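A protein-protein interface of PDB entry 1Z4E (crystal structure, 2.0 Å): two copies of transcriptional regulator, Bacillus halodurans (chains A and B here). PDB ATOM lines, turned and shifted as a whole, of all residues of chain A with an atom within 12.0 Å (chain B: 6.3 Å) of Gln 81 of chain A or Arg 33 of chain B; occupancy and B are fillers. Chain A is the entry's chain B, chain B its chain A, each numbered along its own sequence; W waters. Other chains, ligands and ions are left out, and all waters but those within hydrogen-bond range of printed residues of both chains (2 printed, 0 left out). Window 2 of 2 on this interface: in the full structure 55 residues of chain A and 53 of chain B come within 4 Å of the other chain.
Among the printed residues, merely in contact across the chains: Tyr 77 of chain A with Ala 45 of chain B (3.4 Å), Leu 78 of chain A with Tyr 42 of chain B (3.2 Å), Thr 79 of chain A with Glu 32 of chain B (3.4 Å), Tyr 80 of chain A with Arg 31 of chain B (3.3 Å), Gln 81 of chain A with Tyr 42 of chain B (3.3 Å), Gly 82 of chain A with Ser 41 of chain B (3.8 Å), Gly 82 of chain A with Tyr 42 of chain B (3.8 Å) and Gly 82 of chain A with Ala 45 of chain B (3.5 Å).
No position is printed for both chains.
Gln 81 of chain A touches just these residues of chain B: Arg 31 (3.0 Å), Glu 32 (2.9 Å), Arg 33 (2.9 Å), Ser 41 (3.1 Å) and Tyr 42 (3.3 Å). Ala 23 of chain B touches none of the printed residues of chain A. No residue of chain A comes within 4 Å of Glu 35 of chain B. Of chain A, only Gln 81 (3.1 Å) and Gly 82 (3.8 Å) come within 4 Å of Ser 41 of chain B. Of the printed residues of chain A, Tyr 42 of chain B touches Leu 78 (3.2 Å), Gln 81 (3.3 Å) and Gly 82 (3.8 Å). Of the printed residues of chain A, Arg 31 of chain B touches Tyr 80 (3.3 Å) and Gln 81 (3.0 Å). Of the printed residues of chain B, Tyr 80 of chain A touches Arg 31 and Glu 32. Printed residues of chain A within 4 Å of Ala 45 of chain B: Tyr 77 and Gly 82. Printed residues of chain B within 4 Å of Tyr 77 of chain A: Ala 45 (3.4 Å). Of the printed residues of chain B, Thr 79 of chain A touches Glu 32. Gly 118 of chain A touches none of the printed residues of chain B. Lys 30 of chain B touches none of the printed residues of chain A. The nearest residue of chain B that does not touch Gln 81 of chain A is Pro 39 of chain B (5.3 Å). The nearest printed residue of chain A that does not touch Ala 45 of chain B is Leu 78 of chain A (4.5 Å).
Water W1 lies within hydrogen-bond range of O of Ser 41 of chain B and O of Gly 82 of chain A. Water W2 bridges OG of Ser 41 of chain B (2.7 Å) and OE1 of Gln 81 of chain A (2.7 Å).
O of Tyr 80 of chain A sits at hydrogen-bond distance from OG of Ser 83 of chain A (2.6 Å). The side-chain carboxylate of Glu 32 of chain B lies within hydrogen-bond range of the side-chain hydroxyl of Tyr 42 of chain B (2.4 Å). The backbone NH (N) of Tyr 77 of chain A sits at hydrogen-bond distance from the backbone carbonyl oxygen (O) of Ser 83 of chain A (3.3 Å). N of Arg 33 of chain B is in hydrogen-bond range of OH of Tyr 42 of chain B, 2.9 Å away. The guanidinium group (NH2) of Arg 85 of chain A sits at hydrogen-bond distance from the side-chain hydroxyl (OG1) of Thr 79 of chain A, at 2.8 Å.
The side-chain carboxylate (OE2) of Glu 32 of chain B sits at hydrogen-bond distance from the backbone NH (N) of Tyr 80 of chain A, at 2.7 Å. The backbone carbonyl oxygen of Arg 31 of chain B sits at hydrogen-bond distance from the side-chain amide nitrogen of Gln 81 of chain A, 3.0 Å away. The guanidinium group of Arg 33 of chain B sits at hydrogen-bond distance from the side-chain amide oxygen of Gln 81 of chain A, 2.9 Å away. The side-chain hydroxyl of Ser 41 of chain B sits at hydrogen-bond distance from the backbone carbonyl oxygen of Gln 81 of chain A (3.1 Å). The side-chain carboxylate (OE1) of Glu 32 of chain B is in hydrogen-bond range of the backbone NH (N) of Gln 81 of chain A, at 2.9 Å.
Of the 15 printed residues of chain A, 6 touch a printed residue of chain B. Printed residues of chain A that touch a printed residue of chain B: Tyr 77, Leu 78, Thr 79, Tyr 80, Gln 81 and Gly 82. Hydrophobic or aromatic side chains of chain A that line the printed part of chain B: Leu 78 and Tyr 80. Among the printed residues, 13 pairs touch across the chains.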
ATOM      1  N   THR A  75      -9.859  21.486  -7.610  1.00  0.00           N
ATOM      2  CA  THR A  75      -8.600  21.246  -8.298  1.00  0.00           C
ATOM      3  C   THR A  75      -7.527  20.605  -7.430  1.00  0.00           C
ATOM      4  O   THR A  75      -7.422  20.907  -6.236  1.00  0.00           O
ATOM      5  CB  THR A  75      -8.044  22.594  -8.819  1.00  0.00           C
ATOM      6  OG1 THR A  75      -9.048  23.248  -9.603  1.00  0.00           O
ATOM      7  CG2 THR A  75      -6.785  22.381  -9.681  1.00  0.00           C
ATOM      8  N   PRO A  76      -6.727  19.692  -8.014  1.00  0.00           N
ATOM      9  CA  PRO A  76      -5.649  19.030  -7.269  1.00  0.00           C
ATOM     10  C   PRO A  76      -4.378  19.874  -7.386  1.00  0.00           C
ATOM     11  O   PRO A  76      -4.110  20.460  -8.441  1.00  0.00           O
ATOM     12  CB  PRO A  76      -5.503  17.697  -7.988  1.00  0.00           C
ATOM     13  CG  PRO A  76      -5.772  18.079  -9.426  1.00  0.00           C
ATOM     14  CD  PRO A  76      -6.974  19.006  -9.300  1.00  0.00           C
ATOM     15  N   TYR A  77      -3.607  19.953  -6.307  1.00  0.00           N
ATOM     16  CA  TYR A  77      -2.358  20.717  -6.310  1.00  0.00           C
ATOM     17  C   TYR A  77      -1.276  19.894  -5.604  1.00  0.00           C
ATOM     18  O   TYR A  77      -1.592  18.974  -4.846  1.00  0.00           O
ATOM     19  CB  TYR A  77      -2.523  22.030  -5.540  1.00  0.00           C
ATOM     20  CG  TYR A  77      -3.561  22.984  -6.081  1.00  0.00           C
ATOM     21  CD1 TYR A  77      -3.211  24.012  -6.963  1.00  0.00           C
ATOM     22  CD2 TYR A  77      -4.893  22.876  -5.691  1.00  0.00           C
ATOM     23  CE1 TYR A  77      -4.178  24.916  -7.439  1.00  0.00           C
ATOM     24  CE2 TYR A  77      -5.857  23.763  -6.153  1.00  0.00           C
ATOM     25  CZ  TYR A  77      -5.499  24.777  -7.020  1.00  0.00           C
ATOM     26  OH  TYR A  77      -6.470  25.646  -7.448  1.00  0.00           O
ATOM     27  N   LEU A  78      -0.010  20.228  -5.854  1.00  0.00           N
ATOM     28  CA  LEU A  78       1.102  19.550  -5.191  1.00  0.00           C
ATOM     29  C   LEU A  78       1.254  20.079  -3.768  1.00  0.00           C
ATOM     30  O   LEU A  78       1.634  19.339  -2.866  1.00  0.00           O
ATOM     31  CB  LEU A  78       2.425  19.797  -5.918  1.00  0.00           C
ATOM     32  CG  LEU A  78       2.926  18.809  -6.964  1.00  0.00           C
ATOM     33  CD1 LEU A  78       4.390  19.125  -7.253  1.00  0.00           C
ATOM     34  CD2 LEU A  78       2.787  17.374  -6.459  1.00  0.00           C
ATOM     35  N   THR A  79       0.968  21.368  -3.583  1.00  0.00           N
ATOM     36  CA  THR A  79       1.085  22.016  -2.274  1.00  0.00           C
ATOM     37  C   THR A  79       0.174  21.409  -1.213  1.00  0.00           C
ATOM     38  O   THR A  79      -0.860  20.816  -1.528  1.00  0.00           O
ATOM     39  CB  THR A  79       0.785  23.531  -2.374  1.00  0.00           C
ATOM     40  OG1 THR A  79      -0.419  23.732  -3.122  1.00  0.00           O
ATOM     41  CG2 THR A  79       1.937  24.259  -3.058  1.00  0.00           C
ATOM     42  N   TYR A  80       0.564  21.572   0.049  1.00  0.00           N
ATOM     43  CA  TYR A  80      -0.196  21.029   1.166  1.00  0.00           C
ATOM     44  C   TYR A  80      -0.241  19.516   1.043  1.00  0.00           C
ATOM     45  O   TYR A  80      -1.280  18.882   1.253  1.00  0.00           O
ATOM     46  CB  TYR A  80      -1.607  21.620   1.184  1.00  0.00           C
ATOM     47  CG  TYR A  80      -1.629  23.042   1.691  1.00  0.00           C
ATOM     48  CD1 TYR A  80      -1.489  23.313   3.051  1.00  0.00           C
ATOM     49  CD2 TYR A  80      -1.741  24.118   0.811  1.00  0.00           C
ATOM     50  CE1 TYR A  80      -1.457  24.620   3.524  1.00  0.00           C
ATOM     51  CE2 TYR A  80      -1.708  25.435   1.277  1.00  0.00           C
ATOM     52  CZ  TYR A  80      -1.564  25.673   2.636  1.00  0.00           C
ATOM     53  OH  TYR A  80      -1.527  26.962   3.116  1.00  0.00           O
ATOM     54  N   GLN A  81       0.907  18.946   0.691  1.00  0.00           N
ATOM     55  CA  GLN A  81       1.033  17.508   0.538  1.00  0.00           C
ATOM     56  C   GLN A  81      -0.007  16.951  -0.428  1.00  0.00           C
ATOM     57  O   GLN A  81      -0.718  15.998  -0.113  1.00  0.00           O
ATOM     58  CB  GLN A  81       0.921  16.836   1.913  1.00  0.00           C
ATOM     59  CG  GLN A  81       1.986  17.318   2.889  1.00  0.00           C
ATOM     60  CD  GLN A  81       1.859  16.699   4.270  1.00  0.00           C
ATOM     61  OE1 GLN A  81       1.854  15.477   4.419  1.00  0.00           O
ATOM     62  NE2 GLN A  81       1.762  17.544   5.289  1.00  0.00           N
ATOM     63  N   GLY A  82      -0.098  17.563  -1.608  1.00  0.00           N
ATOM     64  CA  GLY A  82      -1.040  17.101  -2.616  1.00  0.00           C
ATOM     65  C   GLY A  82      -2.508  17.293  -2.287  1.00  0.00           C
ATOM     66  O   GLY A  82      -3.342  16.454  -2.630  1.00  0.00           O
ATOM     67  N   SER A  83      -2.835  18.405  -1.641  1.00  0.00           N
ATOM     68  CA  SER A  83      -4.220  18.677  -1.269  1.00  0.00           C
ATOM     69  C   SER A  83      -5.063  19.289  -2.380  1.00  0.00           C
ATOM     70  O   SER A  83      -4.595  20.136  -3.144  1.00  0.00           O
ATOM     71  CB  SER A  83      -4.269  19.608  -0.051  1.00  0.00           C
ATOM     72  OG  SER A  83      -3.875  18.935   1.132  1.00  0.00           O
ATOM     73  N   TRP A  84      -6.310  18.836  -2.471  1.00  0.00           N
ATOM     74  CA  TRP A  84      -7.244  19.387  -3.437  1.00  0.00           C
ATOM     75  C   TRP A  84      -7.815  20.638  -2.783  1.00  0.00           C
ATOM     76  O   TRP A  84      -7.974  20.684  -1.563  1.00  0.00           O
ATOM     77  CB  TRP A  84      -8.402  18.427  -3.706  1.00  0.00           C
ATOM     78  CG  TRP A  84      -8.140  17.383  -4.732  1.00  0.00           C
ATOM     79  CD1 TRP A  84      -7.268  16.341  -4.639  1.00  0.00           C
ATOM     80  CD2 TRP A  84      -8.802  17.244  -5.996  1.00  0.00           C
ATOM     81  NE1 TRP A  84      -7.346  15.553  -5.767  1.00  0.00           N
ATOM     82  CE2 TRP A  84      -8.280  16.086  -6.615  1.00  0.00           C
ATOM     83  CE3 TRP A  84      -9.786  17.985  -6.664  1.00  0.00           C
ATOM     84  CZ2 TRP A  84      -8.711  15.649  -7.873  1.00  0.00           C
ATOM     85  CZ3 TRP A  84     -10.215  17.551  -7.918  1.00  0.00           C
ATOM     86  CH2 TRP A  84      -9.675  16.391  -8.508  1.00  0.00           C
ATOM     87  N   ARG A  85      -8.119  21.646  -3.588  1.00  0.00           N
ATOM     88  CA  ARG A  85      -8.699  22.878  -3.070  1.00  0.00           C
ATOM     89  C   ARG A  85      -9.958  23.203  -3.852  1.00  0.00           C
ATOM     90  O   ARG A  85     -10.092  22.835  -5.024  1.00  0.00           O
ATOM     91  CB  ARG A  85      -7.748  24.069  -3.235  1.00  0.00           C
ATOM     92  CG  ARG A  85      -6.367  23.926  -2.638  1.00  0.00           C
ATOM     93  CD  ARG A  85      -5.628  25.258  -2.757  1.00  0.00           C
ATOM     94  NE  ARG A  85      -4.185  25.107  -2.596  1.00  0.00           N
ATOM     95  CZ  ARG A  85      -3.333  26.121  -2.494  1.00  0.00           C
ATOM     96  NH1 ARG A  85      -3.779  27.371  -2.533  1.00  0.00           N
ATOM     97  NH2 ARG A  85      -2.035  25.887  -2.347  1.00  0.00           N
ATOM     98  N   GLY A 118     -13.413  16.072  -0.723  1.00  0.00           N
ATOM     99  CA  GLY A 118     -12.104  15.742  -0.192  1.00  0.00           C
ATOM    100  C   GLY A 118     -11.120  16.898  -0.212  1.00  0.00           C
ATOM    101  O   GLY A 118      -9.913  16.694  -0.078  1.00  0.00           O
ATOM    102  N   CYS A 119     -11.625  18.116  -0.378  1.00  0.00           N
ATOM    103  CA  CYS A 119     -10.756  19.287  -0.383  1.00  0.00           C
ATOM    104  C   CYS A 119     -10.335  19.582   1.050  1.00  0.00           C
ATOM    105  O   CYS A 119     -11.084  19.317   1.989  1.00  0.00           O
ATOM    106  CB  CYS A 119     -11.493  20.497  -0.967  1.00  0.00           C
ATOM    107  SG  CYS A 119     -11.919  20.325  -2.708  1.00  0.00           S
ATOM    108  N   HIS A 120      -9.134  20.123   1.221  1.00  0.00           N
ATOM    109  CA  HIS A 120      -8.640  20.441   2.555  1.00  0.00           C
ATOM    110  C   HIS A 120      -8.669  21.946   2.786  1.00  0.00           C
ATOM    111  O   HIS A 120      -8.421  22.427   3.892  1.00  0.00           O
ATOM    112  CB  HIS A 120      -7.212  19.905   2.731  1.00  0.00           C
ATOM    113  CG  HIS A 120      -7.124  18.406   2.731  1.00  0.00           C
ATOM    114  ND1 HIS A 120      -5.924  17.730   2.719  1.00  0.00           N
ATOM    115  CD2 HIS A 120      -8.090  17.456   2.750  1.00  0.00           C
ATOM    116  CE1 HIS A 120      -6.152  16.428   2.729  1.00  0.00           C
ATOM    117  NE2 HIS A 120      -7.459  16.236   2.749  1.00  0.00           N
ATOM    118  N   LEU A 121      -9.001  22.682   1.731  1.00  0.00           N
ATOM    119  CA  LEU A 121      -9.053  24.136   1.794  1.00  0.00           C
ATOM    120  C   LEU A 121     -10.030  24.700   0.755  1.00  0.00           C
ATOM    121  O   LEU A 121     -10.215  24.117  -0.309  1.00  0.00           O
ATOM    122  CB  LEU A 121      -7.641  24.680   1.546  1.00  0.00           C
ATOM    123  CG  LEU A 121      -7.407  26.110   1.067  1.00  0.00           C
ATOM    124  CD1 LEU A 121      -7.928  27.105   2.091  1.00  0.00           C
ATOM    125  CD2 LEU A 121      -5.911  26.307   0.840  1.00  0.00           C
ATOM    126  N   VAL B  19       9.115  18.543  -4.619  1.00  0.00           N
ATOM    127  CA  VAL B  19       8.665  18.392  -3.233  1.00  0.00           C
ATOM    128  C   VAL B  19       9.694  19.008  -2.284  1.00  0.00           C
ATOM    129  O   VAL B  19       9.330  19.681  -1.321  1.00  0.00           O
ATOM    130  CB  VAL B  19       8.456  16.903  -2.851  1.00  0.00           C
ATOM    131  CG1 VAL B  19       8.059  16.786  -1.373  1.00  0.00           C
ATOM    132  CG2 VAL B  19       7.376  16.292  -3.728  1.00  0.00           C
ATOM    133  N   ALA B  23       8.966  21.997   0.437  1.00  0.00           N
ATOM    134  CA  ALA B  23       9.249  21.832   1.860  1.00  0.00           C
ATOM    135  C   ALA B  23      10.295  22.813   2.375  1.00  0.00           C
ATOM    136  O   ALA B  23      10.328  23.123   3.565  1.00  0.00           O
ATOM    137  CB  ALA B  23       9.705  20.405   2.137  1.00  0.00           C
ATOM    138  N   GLY B  28       6.040  26.959   3.252  1.00  0.00           N
ATOM    139  CA  GLY B  28       5.724  25.573   2.956  1.00  0.00           C
ATOM    140  C   GLY B  28       6.350  24.616   3.953  1.00  0.00           C
ATOM    141  O   GLY B  28       5.855  23.512   4.175  1.00  0.00           O
ATOM    142  N   ARG B  29       7.447  25.050   4.557  1.00  0.00           N
ATOM    143  CA  ARG B  29       8.164  24.248   5.534  1.00  0.00           C
ATOM    144  C   ARG B  29       7.216  23.774   6.633  1.00  0.00           C
ATOM    145  O   ARG B  29       7.392  22.695   7.201  1.00  0.00           O
ATOM    146  CB  ARG B  29       9.295  25.090   6.121  1.00  0.00           C
ATOM    147  CG  ARG B  29      10.251  24.365   7.042  1.00  0.00           C
ATOM    148  CD  ARG B  29      11.548  25.160   7.141  1.00  0.00           C
ATOM    149  NE  ARG B  29      11.293  26.576   7.399  1.00  0.00           N
ATOM    150  CZ  ARG B  29      12.198  27.540   7.254  1.00  0.00           C
ATOM    151  NH1 ARG B  29      13.428  27.245   6.846  1.00  0.00           N
ATOM    152  NH2 ARG B  29      11.875  28.801   7.515  1.00  0.00           N
ATOM    153  N   LYS B  30       6.191  24.578   6.902  1.00  0.00           N
ATOM    154  CA  LYS B  30       5.212  24.269   7.938  1.00  0.00           C
ATOM    155  C   LYS B  30       4.040  23.424   7.441  1.00  0.00           C
ATOM    156  O   LYS B  30       3.295  22.863   8.242  1.00  0.00           O
ATOM    157  CB  LYS B  30       4.657  25.571   8.529  1.00  0.00           C
ATOM    158  CG  LYS B  30       5.696  26.490   9.165  1.00  0.00           C
ATOM    159  CD  LYS B  30       6.285  25.882  10.434  1.00  0.00           C
ATOM    160  CE  LYS B  30       7.256  26.840  11.118  1.00  0.00           C
ATOM    161  NZ  LYS B  30       8.437  27.168  10.266  1.00  0.00           N
ATOM    162  N   ARG B  31       3.883  23.324   6.126  1.00  0.00           N
ATOM    163  CA  ARG B  31       2.761  22.582   5.559  1.00  0.00           C
ATOM    164  C   ARG B  31       3.129  21.341   4.750  1.00  0.00           C
ATOM    165  O   ARG B  31       2.302  20.448   4.567  1.00  0.00           O
ATOM    166  CB  ARG B  31       1.937  23.519   4.675  1.00  0.00           C
ATOM    167  CG  ARG B  31       1.353  24.731   5.393  1.00  0.00           C
ATOM    168  CD  ARG B  31       0.216  24.337   6.333  1.00  0.00           C
ATOM    169  NE  ARG B  31      -0.559  25.499   6.770  1.00  0.00           N
ATOM    170  CZ  ARG B  31      -1.723  25.428   7.411  1.00  0.00           C
ATOM    171  NH1 ARG B  31      -2.255  24.246   7.697  1.00  0.00           N
ATOM    172  NH2 ARG B  31      -2.360  26.540   7.761  1.00  0.00           N
ATOM    173  N   GLU B  32       4.360  21.283   4.262  1.00  0.00           N
ATOM    174  CA  GLU B  32       4.786  20.155   3.445  1.00  0.00           C
ATOM    175  C   GLU B  32       5.469  19.042   4.233  1.00  0.00           C
ATOM    176  O   GLU B  32       5.759  19.182   5.420  1.00  0.00           O
ATOM    177  CB  GLU B  32       5.724  20.647   2.339  1.00  0.00           C
ATOM    178  CG  GLU B  32       5.160  21.783   1.498  1.00  0.00           C
ATOM    179  CD  GLU B  32       3.853  21.421   0.803  1.00  0.00           C
ATOM    180  OE1 GLU B  32       3.563  20.218   0.626  1.00  0.00           O
ATOM    181  OE2 GLU B  32       3.118  22.345   0.419  1.00  0.00           O
ATOM    182  N   ARG B  33       5.718  17.926   3.558  1.00  0.00           N
ATOM    183  CA  ARG B  33       6.377  16.793   4.188  1.00  0.00           C
ATOM    184  C   ARG B  33       7.360  16.176   3.208  1.00  0.00           C
ATOM    185  O   ARG B  33       6.999  15.317   2.405  1.00  0.00           O
ATOM    186  CB  ARG B  33       5.348  15.745   4.613  1.00  0.00           C
ATOM    187  CG  ARG B  33       5.938  14.566   5.381  1.00  0.00           C
ATOM    188  CD  ARG B  33       4.909  13.456   5.566  1.00  0.00           C
ATOM    189  NE  ARG B  33       3.652  13.963   6.112  1.00  0.00           N
ATOM    190  CZ  ARG B  33       3.531  14.557   7.295  1.00  0.00           C
ATOM    191  NH1 ARG B  33       4.595  14.722   8.070  1.00  0.00           N
ATOM    192  NH2 ARG B  33       2.345  14.995   7.704  1.00  0.00           N
ATOM    193  N   TYR B  34       8.605  16.629   3.260  1.00  0.00           N
ATOM    194  CA  TYR B  34       9.619  16.080   2.380  1.00  0.00           C
ATOM    195  C   TYR B  34      10.318  14.919   3.073  1.00  0.00           C
ATOM    196  O   TYR B  34      10.766  15.044   4.212  1.00  0.00           O
ATOM    197  CB  TYR B  34      10.670  17.125   2.020  1.00  0.00           C
ATOM    198  CG  TYR B  34      11.816  16.540   1.218  1.00  0.00           C
ATOM    199  CD1 TYR B  34      11.648  16.186  -0.123  1.00  0.00           C
ATOM    200  CD2 TYR B  34      13.060  16.312   1.808  1.00  0.00           C
ATOM    201  CE1 TYR B  34      12.696  15.622  -0.859  1.00  0.00           C
ATOM    202  CE2 TYR B  34      14.111  15.748   1.084  1.00  0.00           C
ATOM    203  CZ  TYR B  34      13.923  15.408  -0.248  1.00  0.00           C
ATOM    204  OH  TYR B  34      14.961  14.863  -0.967  1.00  0.00           O
ATOM    205  N   GLU B  35      10.392  13.790   2.382  1.00  0.00           N
ATOM    206  CA  GLU B  35      11.081  12.624   2.902  1.00  0.00           C
ATOM    207  C   GLU B  35      11.277  11.624   1.766  1.00  0.00           C
ATOM    208  O   GLU B  35      10.686  11.770   0.691  1.00  0.00           O
ATOM    209  CB  GLU B  35      10.298  12.005   4.067  1.00  0.00           C
ATOM    210  CG  GLU B  35       8.935  11.441   3.730  1.00  0.00           C
ATOM    211  CD  GLU B  35       8.089  11.209   4.975  1.00  0.00           C
ATOM    212  OE1 GLU B  35       7.139  10.402   4.914  1.00  0.00           O
ATOM    213  OE2 GLU B  35       8.368  11.848   6.014  1.00  0.00           O
ATOM    214  N   LEU B  38       9.091   9.500  -1.097  1.00  0.00           N
ATOM    215  CA  LEU B  38       8.143  10.614  -1.091  1.00  0.00           C
ATOM    216  C   LEU B  38       6.756  10.155  -0.635  1.00  0.00           C
ATOM    217  O   LEU B  38       6.327   9.041  -0.953  1.00  0.00           O
ATOM    218  CB  LEU B  38       8.032  11.209  -2.501  1.00  0.00           C
ATOM    219  CG  LEU B  38       9.301  11.790  -3.140  1.00  0.00           C
ATOM    220  CD1 LEU B  38       9.048  12.078  -4.617  1.00  0.00           C
ATOM    221  CD2 LEU B  38       9.709  13.064  -2.405  1.00  0.00           C
ATOM    222  N   PRO B  39       6.040  11.003   0.127  1.00  0.00           N
ATOM    223  CA  PRO B  39       4.698  10.642   0.597  1.00  0.00           C
ATOM    224  C   PRO B  39       3.793  10.403  -0.612  1.00  0.00           C
ATOM    225  O   PRO B  39       3.809  11.185  -1.566  1.00  0.00           O
ATOM    226  CB  PRO B  39       4.275  11.868   1.405  1.00  0.00           C
ATOM    227  CG  PRO B  39       5.582  12.380   1.945  1.00  0.00           C
ATOM    228  CD  PRO B  39       6.490  12.267   0.738  1.00  0.00           C
ATOM    229  N   SER B  41       0.797  10.943  -1.068  1.00  0.00           N
ATOM    230  CA  SER B  41      -0.153  12.028  -1.301  1.00  0.00           C
ATOM    231  C   SER B  41       0.332  12.938  -2.436  1.00  0.00           C
ATOM    232  O   SER B  41      -0.473  13.422  -3.231  1.00  0.00           O
ATOM    233  CB  SER B  41      -0.349  12.847  -0.022  1.00  0.00           C
ATOM    234  OG  SER B  41       0.865  13.441   0.396  1.00  0.00           O
ATOM    235  N   TYR B  42       1.641  13.169  -2.515  1.00  0.00           N
ATOM    236  CA  TYR B  42       2.198  14.008  -3.582  1.00  0.00           C
ATOM    237  C   TYR B  42       2.085  13.270  -4.910  1.00  0.00           C
ATOM    238  O   TYR B  42       1.847  13.874  -5.959  1.00  0.00           O
ATOM    239  CB  TYR B  42       3.676  14.330  -3.326  1.00  0.00           C
ATOM    240  CG  TYR B  42       3.937  15.326  -2.216  1.00  0.00           C
ATOM    241  CD1 TYR B  42       3.565  16.663  -2.348  1.00  0.00           C
ATOM    242  CD2 TYR B  42       4.563  14.930  -1.034  1.00  0.00           C
ATOM    243  CE1 TYR B  42       3.812  17.583  -1.328  1.00  0.00           C
ATOM    244  CE2 TYR B  42       4.811  15.837  -0.007  1.00  0.00           C
ATOM    245  CZ  TYR B  42       4.435  17.162  -0.159  1.00  0.00           C
ATOM    246  OH  TYR B  42       4.684  18.056   0.855  1.00  0.00           O
ATOM    247  N   ALA B  45      -1.511  13.329  -6.250  1.00  0.00           N
ATOM    248  CA  ALA B  45      -1.803  14.659  -6.769  1.00  0.00           C
ATOM    249  C   ALA B  45      -1.131  14.841  -8.127  1.00  0.00           C
ATOM    250  O   ALA B  45      -1.742  15.355  -9.062  1.00  0.00           O
ATOM    251  CB  ALA B  45      -1.317  15.734  -5.784  1.00  0.00           C
HETATM  252  O   HOH W   1      -3.127  13.712  -2.923  1.00  0.00           O
HETATM  253  O   HOH W   2       1.188  13.198   3.082  1.00  0.00           O
